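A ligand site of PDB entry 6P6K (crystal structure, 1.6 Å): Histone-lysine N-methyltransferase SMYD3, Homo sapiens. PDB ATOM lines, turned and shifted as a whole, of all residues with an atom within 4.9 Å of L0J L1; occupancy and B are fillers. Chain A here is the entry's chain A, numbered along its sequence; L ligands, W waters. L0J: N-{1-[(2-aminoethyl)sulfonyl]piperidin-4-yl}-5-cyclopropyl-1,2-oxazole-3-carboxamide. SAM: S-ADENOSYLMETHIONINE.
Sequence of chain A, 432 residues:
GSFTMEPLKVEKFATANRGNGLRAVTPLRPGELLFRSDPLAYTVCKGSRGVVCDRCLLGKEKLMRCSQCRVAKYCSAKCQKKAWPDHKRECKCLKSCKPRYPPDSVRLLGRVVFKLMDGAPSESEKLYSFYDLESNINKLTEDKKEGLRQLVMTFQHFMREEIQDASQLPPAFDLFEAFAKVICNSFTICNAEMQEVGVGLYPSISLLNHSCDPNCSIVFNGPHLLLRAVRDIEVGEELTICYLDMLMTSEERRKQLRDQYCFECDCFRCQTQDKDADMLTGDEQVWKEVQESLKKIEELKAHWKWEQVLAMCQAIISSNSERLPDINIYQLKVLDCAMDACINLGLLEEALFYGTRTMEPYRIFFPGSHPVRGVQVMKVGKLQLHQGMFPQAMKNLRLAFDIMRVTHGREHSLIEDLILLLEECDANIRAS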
ATOM      1  N   CYS A 184     -30.686  19.901  15.316  1.00  0.00           N
ATOM      2  CA  CYS A 184     -30.218  20.245  13.983  1.00  0.00           C
ATOM      3  C   CYS A 184     -28.699  20.236  13.863  1.00  0.00           C
ATOM      4  O   CYS A 184     -28.164  20.775  12.895  1.00  0.00           O
ATOM      5  CB  CYS A 184     -30.796  21.601  13.549  1.00  0.00           C
ATOM      6  SG  CYS A 184     -30.361  23.050  14.543  1.00  0.00           S
ATOM      7  N   ASN A 185     -28.007  19.618  14.825  1.00  0.00           N
ATOM      8  CA  ASN A 185     -26.551  19.539  14.756  1.00  0.00           C
ATOM      9  C   ASN A 185     -26.002  18.167  15.140  1.00  0.00           C
ATOM     10  O   ASN A 185     -24.810  18.051  15.426  1.00  0.00           O
ATOM     11  CB  ASN A 185     -25.929  20.612  15.644  1.00  0.00           C
ATOM     12  CG  ASN A 185     -26.085  21.991  15.067  1.00  0.00           C
ATOM     13  OD1 ASN A 185     -25.357  22.376  14.141  1.00  0.00           O
ATOM     14  ND2 ASN A 185     -27.041  22.767  15.616  1.00  0.00           N
ATOM     15  N   SER A 186     -26.837  17.140  15.166  1.00  0.00           N
ATOM     16  CA  SER A 186     -26.396  15.810  15.586  1.00  0.00           C
ATOM     17  C   SER A 186     -25.832  15.053  14.392  1.00  0.00           C
ATOM     18  O   SER A 186     -26.487  14.927  13.355  1.00  0.00           O
ATOM     19  CB  SER A 186     -27.532  15.018  16.204  1.00  0.00           C
ATOM     20  OG  SER A 186     -27.881  15.551  17.468  1.00  0.00           O
ATOM     21  N   PHE A 187     -24.635  14.513  14.570  1.00  0.00           N
ATOM     22  CA  PHE A 187     -23.990  13.680  13.566  1.00  0.00           C
ATOM     23  C   PHE A 187     -24.236  12.207  13.874  1.00  0.00           C
ATOM     24  O   PHE A 187     -24.017  11.756  15.007  1.00  0.00           O
ATOM     25  CB  PHE A 187     -22.498  13.972  13.515  1.00  0.00           C
ATOM     26  CG  PHE A 187     -22.168  15.302  12.872  1.00  0.00           C
ATOM     27  CD1 PHE A 187     -22.187  16.469  13.631  1.00  0.00           C
ATOM     28  CD2 PHE A 187     -21.871  15.374  11.522  1.00  0.00           C
ATOM     29  CE1 PHE A 187     -21.889  17.695  13.039  1.00  0.00           C
ATOM     30  CE2 PHE A 187     -21.574  16.604  10.921  1.00  0.00           C
ATOM     31  CZ  PHE A 187     -21.590  17.763  11.697  1.00  0.00           C
ATOM     32  N   THR A 188     -24.672  11.461  12.860  1.00  0.00           N
ATOM     33  CA  THR A 188     -24.890  10.030  12.994  1.00  0.00           C
ATOM     34  C   THR A 188     -23.563   9.311  12.744  1.00  0.00           C
ATOM     35  O   THR A 188     -23.084   9.261  11.613  1.00  0.00           O
ATOM     36  CB  THR A 188     -25.965   9.562  12.014  1.00  0.00           C
ATOM     37  OG1 THR A 188     -27.167  10.303  12.270  1.00  0.00           O
ATOM     38  CG2 THR A 188     -26.246   8.081  12.209  1.00  0.00           C
ATOM     39  N   CYS A 190     -21.104   6.350  12.180  1.00  0.00           N
ATOM     40  CA  CYS A 190     -21.155   5.036  11.570  1.00  0.00           C
ATOM     41  C   CYS A 190     -19.808   4.343  11.695  1.00  0.00           C
ATOM     42  O   CYS A 190     -18.764   4.986  11.669  1.00  0.00           O
ATOM     43  CB  CYS A 190     -21.544   5.117  10.096  1.00  0.00           C
ATOM     44  SG  CYS A 190     -23.165   5.829   9.824  1.00  0.00           S
ATOM     45  N   MET A 194     -20.190   0.961   7.894  1.00  0.00           N
ATOM     46  CA  MET A 194     -21.249   1.930   7.615  1.00  0.00           C
ATOM     47  C   MET A 194     -22.535   1.645   8.380  1.00  0.00           C
ATOM     48  O   MET A 194     -23.604   2.116   7.991  1.00  0.00           O
ATOM     49  CB  MET A 194     -21.521   2.035   6.115  1.00  0.00           C
ATOM     50  CG  MET A 194     -20.424   2.776   5.408  1.00  0.00           C
ATOM     51  SD  MET A 194     -20.290   4.446   6.091  1.00  0.00           S
ATOM     52  CE  MET A 194     -18.836   5.037   5.237  1.00  0.00           C
ATOM     53  N   GLU A 196     -24.764   2.461  11.576  1.00  0.00           N
ATOM     54  CA  GLU A 196     -24.928   3.511  12.575  1.00  0.00           C
ATOM     55  C   GLU A 196     -24.683   2.939  13.960  1.00  0.00           C
ATOM     56  O   GLU A 196     -25.306   1.946  14.351  1.00  0.00           O
ATOM     57  CB  GLU A 196     -26.319   4.112  12.466  1.00  0.00           C
ATOM     58  CG  GLU A 196     -26.651   4.576  11.059  1.00  0.00           C
ATOM     59  CD  GLU A 196     -28.057   5.109  10.915  1.00  0.00           C
ATOM     60  OE1 GLU A 196     -28.682   5.432  11.946  1.00  0.00           O
ATOM     61  OE2 GLU A 196     -28.543   5.209   9.770  1.00  0.00           O
ATOM     62  N   SER A 206     -20.183  21.400  12.300  1.00  0.00           N
ATOM     63  CA  SER A 206     -21.539  21.898  12.177  1.00  0.00           C
ATOM     64  C   SER A 206     -21.642  23.137  11.315  1.00  0.00           C
ATOM     65  O   SER A 206     -22.758  23.560  11.021  1.00  0.00           O
ATOM     66  CB  SER A 206     -22.111  22.215  13.562  1.00  0.00           C
ATOM     67  OG  SER A 206     -22.802  21.097  14.089  1.00  0.00           O
ATOM     68  N   ILE A 218     -18.105  13.489   4.928  1.00  0.00           N
ATOM     69  CA  ILE A 218     -17.523  13.088   6.210  1.00  0.00           C
ATOM     70  C   ILE A 218     -17.551  11.568   6.318  1.00  0.00           C
ATOM     71  O   ILE A 218     -18.415  10.888   5.757  1.00  0.00           O
ATOM     72  CB  ILE A 218     -18.227  13.717   7.423  1.00  0.00           C
ATOM     73  CG1 ILE A 218     -19.688  13.280   7.484  1.00  0.00           C
ATOM     74  CG2 ILE A 218     -18.101  15.235   7.357  1.00  0.00           C
ATOM     75  CD1 ILE A 218     -20.404  13.703   8.761  1.00  0.00           C
ATOM     76  N   PHE A 220     -16.430   8.451   9.431  1.00  0.00           N
ATOM     77  CA  PHE A 220     -16.056   8.215  10.814  1.00  0.00           C
ATOM     78  C   PHE A 220     -15.092   7.054  10.892  1.00  0.00           C
ATOM     79  O   PHE A 220     -15.260   6.038  10.214  1.00  0.00           O
ATOM     80  CB  PHE A 220     -17.286   7.929  11.663  1.00  0.00           C
ATOM     81  CG  PHE A 220     -18.226   9.072  11.709  1.00  0.00           C
ATOM     82  CD1 PHE A 220     -18.041  10.089  12.646  1.00  0.00           C
ATOM     83  CD2 PHE A 220     -19.280   9.154  10.809  1.00  0.00           C
ATOM     84  CE1 PHE A 220     -18.907  11.159  12.691  1.00  0.00           C
ATOM     85  CE2 PHE A 220     -20.150  10.232  10.858  1.00  0.00           C
ATOM     86  CZ  PHE A 220     -19.968  11.232  11.798  1.00  0.00           C
ATOM     87  N   ILE A 241     -22.007  19.182   2.765  1.00  0.00           N
ATOM     88  CA  ILE A 241     -22.086  17.740   2.931  1.00  0.00           C
ATOM     89  C   ILE A 241     -23.568  17.385   2.834  1.00  0.00           C
ATOM     90  O   ILE A 241     -24.435  18.234   3.002  1.00  0.00           O
ATOM     91  CB  ILE A 241     -21.475  17.267   4.275  1.00  0.00           C
ATOM     92  CG1 ILE A 241     -22.131  17.985   5.459  1.00  0.00           C
ATOM     93  CG2 ILE A 241     -19.960  17.504   4.272  1.00  0.00           C
ATOM     94  CD1 ILE A 241     -21.653  17.444   6.796  1.00  0.00           C
ATOM     95  N   CYS A 242     -23.846  16.126   2.531  1.00  0.00           N
ATOM     96  CA  CYS A 242     -25.225  15.667   2.515  1.00  0.00           C
ATOM     97  C   CYS A 242     -25.574  15.148   3.912  1.00  0.00           C
ATOM     98  O   CYS A 242     -24.972  14.182   4.386  1.00  0.00           O
ATOM     99  CB  CYS A 242     -25.424  14.583   1.453  1.00  0.00           C
ATOM    100  SG  CYS A 242     -27.164  14.123   1.323  1.00  0.00           S
ATOM    101  N   TYR A 243     -26.537  15.801   4.568  1.00  0.00           N
ATOM    102  CA  TYR A 243     -26.922  15.385   5.910  1.00  0.00           C
ATOM    103  C   TYR A 243     -27.619  14.035   5.954  1.00  0.00           C
ATOM    104  O   TYR A 243     -27.791  13.489   7.053  1.00  0.00           O
ATOM    105  CB  TYR A 243     -27.887  16.384   6.543  1.00  0.00           C
ATOM    106  CG  TYR A 243     -27.359  17.760   6.829  1.00  0.00           C
ATOM    107  CD1 TYR A 243     -26.025  18.099   6.596  1.00  0.00           C
ATOM    108  CD2 TYR A 243     -28.197  18.722   7.369  1.00  0.00           C
ATOM    109  CE1 TYR A 243     -25.552  19.384   6.887  1.00  0.00           C
ATOM    110  CE2 TYR A 243     -27.750  19.992   7.656  1.00  0.00           C
ATOM    111  CZ  TYR A 243     -26.436  20.332   7.404  1.00  0.00           C
ATOM    112  OH  TYR A 243     -25.989  21.602   7.690  1.00  0.00           O
ATOM    113  N   LEU A 244     -28.073  13.526   4.817  1.00  0.00           N
ATOM    114  CA  LEU A 244     -29.045  12.440   4.750  1.00  0.00           C
ATOM    115  C   LEU A 244     -28.503  11.247   3.968  1.00  0.00           C
ATOM    116  O   LEU A 244     -27.645  11.376   3.097  1.00  0.00           O
ATOM    117  CB  LEU A 244     -30.314  12.886   4.033  1.00  0.00           C
ATOM    118  CG  LEU A 244     -30.913  14.163   4.593  1.00  0.00           C
ATOM    119  CD1 LEU A 244     -32.129  14.548   3.747  1.00  0.00           C
ATOM    120  CD2 LEU A 244     -31.301  13.917   6.024  1.00  0.00           C
ATOM    121  N   ASP A 245     -29.083  10.091   4.279  1.00  0.00           N
ATOM    122  CA  ASP A 245     -28.945   8.892   3.456  1.00  0.00           C
ATOM    123  C   ASP A 245     -29.277   9.203   1.992  1.00  0.00           C
ATOM    124  O   ASP A 245     -30.268   9.883   1.690  1.00  0.00           O
ATOM    125  CB  ASP A 245     -29.879   7.823   4.040  1.00  0.00           C
ATOM    126  CG  ASP A 245     -30.231   6.695   3.089  1.00  0.00           C
ATOM    127  OD1 ASP A 245     -29.365   6.199   2.356  1.00  0.00           O
ATOM    128  OD2 ASP A 245     -31.416   6.266   3.119  1.00  0.00           O
ATOM    129  N   TYR A 261     -34.263  19.970  10.442  1.00  0.00           N
ATOM    130  CA  TYR A 261     -33.329  21.060  10.153  1.00  0.00           C
ATOM    131  C   TYR A 261     -34.013  22.372   9.812  1.00  0.00           C
ATOM    132  O   TYR A 261     -33.308  23.372   9.607  1.00  0.00           O
ATOM    133  CB  TYR A 261     -32.373  20.664   9.018  1.00  0.00           C
ATOM    134  CG  TYR A 261     -31.514  19.492   9.444  1.00  0.00           C
ATOM    135  CD1 TYR A 261     -30.507  19.674  10.385  1.00  0.00           C
ATOM    136  CD2 TYR A 261     -31.730  18.218   8.944  1.00  0.00           C
ATOM    137  CE1 TYR A 261     -29.712  18.620  10.813  1.00  0.00           C
ATOM    138  CE2 TYR A 261     -30.933  17.139   9.369  1.00  0.00           C
ATOM    139  CZ  TYR A 261     -29.932  17.359  10.286  1.00  0.00           C
ATOM    140  OH  TYR A 261     -29.145  16.316  10.731  1.00  0.00           O
ATOM    141  N   HIS A 370     -18.567   8.592  -3.023  1.00  0.00           N
ATOM    142  CA  HIS A 370     -19.345   8.533  -1.808  1.00  0.00           C
ATOM    143  C   HIS A 370     -18.809   7.408  -0.942  1.00  0.00           C
ATOM    144  O   HIS A 370     -18.617   6.291  -1.446  1.00  0.00           O
ATOM    145  CB  HIS A 370     -20.815   8.305  -2.125  1.00  0.00           C
ATOM    146  CG  HIS A 370     -21.727   8.576  -0.981  1.00  0.00           C
ATOM    147  ND1 HIS A 370     -21.767   7.781   0.142  1.00  0.00           N
ATOM    148  CD2 HIS A 370     -22.644   9.551  -0.787  1.00  0.00           C
ATOM    149  CE1 HIS A 370     -22.673   8.254   0.981  1.00  0.00           C
ATOM    150  NE2 HIS A 370     -23.214   9.341   0.436  1.00  0.00           N
ATOM    151  N   PRO A 371     -18.546   7.653   0.344  1.00  0.00           N
ATOM    152  CA  PRO A 371     -17.967   6.568   1.168  1.00  0.00           C
ATOM    153  C   PRO A 371     -18.832   5.339   1.274  1.00  0.00           C
ATOM    154  O   PRO A 371     -18.312   4.235   1.427  1.00  0.00           O
ATOM    155  CB  PRO A 371     -17.755   7.222   2.537  1.00  0.00           C
ATOM    156  CG  PRO A 371     -18.720   8.402   2.538  1.00  0.00           C
ATOM    157  CD  PRO A 371     -18.719   8.895   1.103  1.00  0.00           C
ATOM    158  N   VAL A 372     -20.162   5.485   1.191  1.00  0.00           N
ATOM    159  CA  VAL A 372     -21.020   4.311   1.280  1.00  0.00           C
ATOM    160  C   VAL A 372     -20.806   3.393   0.093  1.00  0.00           C
ATOM    161  O   VAL A 372     -20.797   2.153   0.240  1.00  0.00           O
ATOM    162  CB  VAL A 372     -22.482   4.738   1.428  1.00  0.00           C
ATOM    163  CG1 VAL A 372     -23.415   3.564   1.197  1.00  0.00           C
ATOM    164  CG2 VAL A 372     -22.679   5.337   2.810  1.00  0.00           C
HETATM  165  C17 L0J L   1     -25.693  10.874   6.637  1.00  0.00           C
HETATM  166  C20 L0J L   1     -25.071  11.085   8.028  1.00  0.00           C
HETATM  167  C22 L0J L   1     -23.736  10.375   8.214  1.00  0.00           C
HETATM  168  C14 L0J L   1     -25.918   9.377   6.453  1.00  0.00           C
HETATM  169  C25 L0J L   1     -24.058   8.891   8.016  1.00  0.00           C
HETATM  170  C30 L0J L   1     -25.088  13.088   9.324  1.00  0.00           C
HETATM  171  C32 L0J L   1     -24.845  14.520   9.324  1.00  0.00           C
HETATM  172  C33 L0J L   1     -25.358  15.533  10.258  1.00  0.00           C
HETATM  173  C35 L0J L   1     -24.853  16.696   9.812  1.00  0.00           C
HETATM  174  C38 L0J L   1     -25.018  18.062  10.374  1.00  0.00           C
HETATM  175  C40 L0J L   1     -25.004  18.204  11.854  1.00  0.00           C
HETATM  176  C43 L0J L   1     -26.274  18.365  11.102  1.00  0.00           C
HETATM  177  N28 L0J L   1     -24.858  12.514   8.156  1.00  0.00           N
HETATM  178  N37 L0J L   1     -24.116  15.109   8.414  1.00  0.00           N
HETATM  179  O31 L0J L   1     -25.432  12.464  10.325  1.00  0.00           O
HETATM  180  O36 L0J L   1     -24.092  16.464   8.686  1.00  0.00           O
HETATM  181  C04 L0J L   1     -25.372   5.473   6.641  1.00  0.00           C
HETATM  182  C07 L0J L   1     -23.960   5.903   6.253  1.00  0.00           C
HETATM  183  N01 L0J L   1     -25.383   4.017   6.860  1.00  0.00           N
HETATM  184  N13 L0J L   1     -24.711   8.622   6.733  1.00  0.00           N
HETATM  185  O11 L0J L   1     -22.719   8.032   5.229  1.00  0.00           O
HETATM  186  O12 L0J L   1     -24.868   7.602   4.372  1.00  0.00           O
HETATM  187  S10 L0J L   1     -24.039   7.561   5.539  1.00  0.00           S
HETATM  188  N   SAM L   2     -26.002  27.320   8.810  1.00  0.00           N
HETATM  189  CA  SAM L   2     -25.695  26.616  10.038  1.00  0.00           C
HETATM  190  C   SAM L   2     -25.291  27.634  11.118  1.00  0.00           C
HETATM  191  O   SAM L   2     -24.819  27.261  12.191  1.00  0.00           O
HETATM  192  OXT SAM L   2     -25.456  28.841  10.906  1.00  0.00           O
HETATM  193  CB  SAM L   2     -24.614  25.569   9.785  1.00  0.00           C
HETATM  194  CG  SAM L   2     -25.207  24.204   9.434  1.00  0.00           C
HETATM  195  SD  SAM L   2     -26.099  23.495  10.858  1.00  0.00           S
HETATM  196  CE  SAM L   2     -25.383  21.845  10.997  1.00  0.00           C
HETATM  197  C5' SAM L   2     -27.703  23.009  10.164  1.00  0.00           C
HETATM  198  C4' SAM L   2     -28.605  24.211   9.907  1.00  0.00           C
HETATM  199  O4' SAM L   2     -28.095  24.993   8.842  1.00  0.00           O
HETATM  200  C3' SAM L   2     -29.990  23.806   9.442  1.00  0.00           C
HETATM  201  O3' SAM L   2     -30.802  23.446  10.527  1.00  0.00           O
HETATM  202  C2' SAM L   2     -30.468  25.028   8.676  1.00  0.00           C
HETATM  203  O2' SAM L   2     -30.826  26.028   9.618  1.00  0.00           O
HETATM  204  C1' SAM L   2     -29.167  25.462   8.032  1.00  0.00           C
HETATM  205  N9  SAM L   2     -28.966  24.860   6.705  1.00  0.00           N
HETATM  206  C8  SAM L   2     -28.144  23.794   6.408  1.00  0.00           C
HETATM  207  N7  SAM L   2     -28.190  23.541   5.079  1.00  0.00           N
HETATM  208  C5  SAM L   2     -29.028  24.441   4.509  1.00  0.00           C
HETATM  209  C6  SAM L   2     -29.436  24.636   3.199  1.00  0.00           C
HETATM  210  N6  SAM L   2     -29.014  23.876   2.193  1.00  0.00           N
HETATM  211  N1  SAM L   2     -30.326  25.647   2.943  1.00  0.00           N
HETATM  212  C2  SAM L   2     -30.783  26.450   3.953  1.00  0.00           C
HETATM  213  N3  SAM L   2     -30.384  26.254   5.252  1.00  0.00           N
HETATM  214  C4  SAM L   2     -29.513  25.273   5.527  1.00  0.00           C
HETATM  215  O   HOH W   1     -22.757  20.207   9.387  1.00  0.00           O
HETATM  216  O   HOH W   2     -26.074   7.431   2.009  1.00  0.00           O
HETATM  217  O   HOH W   3     -28.038  12.975  12.060  1.00  0.00           O
HETATM  218  O   HOH W   4     -22.939  13.814   6.045  1.00  0.00           O
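The backbone NH of Thr 188 is in hydrogen-bond range of an oxygen (O31) of L0J L1.
An oxygen (O31) of L0J L1 sits at hydrogen-bond distance from the side-chain hydroxyl (OG1) of Thr 188 (3.4 Å).
N01 of L0J L1 lies within hydrogen-bond range of O of Met 194.
The backbone carbonyl oxygen of Tyr 243 sits at hydrogen-bond distance from a nitrogen (N28) of L0J L1.
The backbone carbonyl oxygen (O) of Tyr 261 is in hydrogen-bond range of an oxygen (O3') of SAM L2 (2.7 Å).
SG of Cys 184 lies close to ND2 of Asn 185 (3.5 Å).
OG of Ser 206 sits at hydrogen-bond distance from OD1 of Asn 185, 2.9 Å away.
N of Val 372 is in hydrogen-bond range of ND1 of His 370, at 3.0 Å.
The backbone carbonyl oxygen of Leu 244 is in hydrogen-bond range of the side-chain sulfur of Cys 242 (3.3 Å).
O of Cys 184 touches C43 of L0J L1, 3.5 Å away.
Asn 185 touches L0J L1 (C to C40, 3.4 Å).
O of Ser 186 touches C33 of L0J L1, 3.4 Å away.
CE2 of Phe 187 touches O36 of L0J L1, 3.4 Å away.
Cys 190 touches L0J L1.
Ile 218 touches L0J L1 (CD1 to N37, 3.98 Å).
Ile 241 touches L0J L1 (CD1 to O36, 3.2 Å).
Leu 244 touches L0J L1 (C to C17, 3.9 Å).
N of Asp 245 touches C14 of L0J L1, 3.9 Å away.
CE1 of Tyr 261 touches C43 of L0J L1 (3.5 Å).
Val 372 touches L0J L1.
Hydrophobic or aromatic side chains that line L0J L1: Phe 187, Met 194, Ile 218, Ile 241, Tyr 243, Tyr 261 and Val 372.
Within 4 Å of L0J L1: Cys 184, Asn 185, Ser 186, Phe 187, Thr 188, Cys 190, Met 194, Ile 218, Ile 241, Tyr 243, Leu 244, Asp 245, Tyr 261 and Val 372.
The nearest printed residue that does not touch L0J L1 is Cys 242 (4.1 Å).
Water W4 bridges O of Cys 242 and N37 of L0J L1.
Water W3 lies within hydrogen-bond range of O of Ser 186 (2.8 Å), OG1 of Thr 188 (2.8 Å) and O31 of L0J L1 (3.2 Å).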
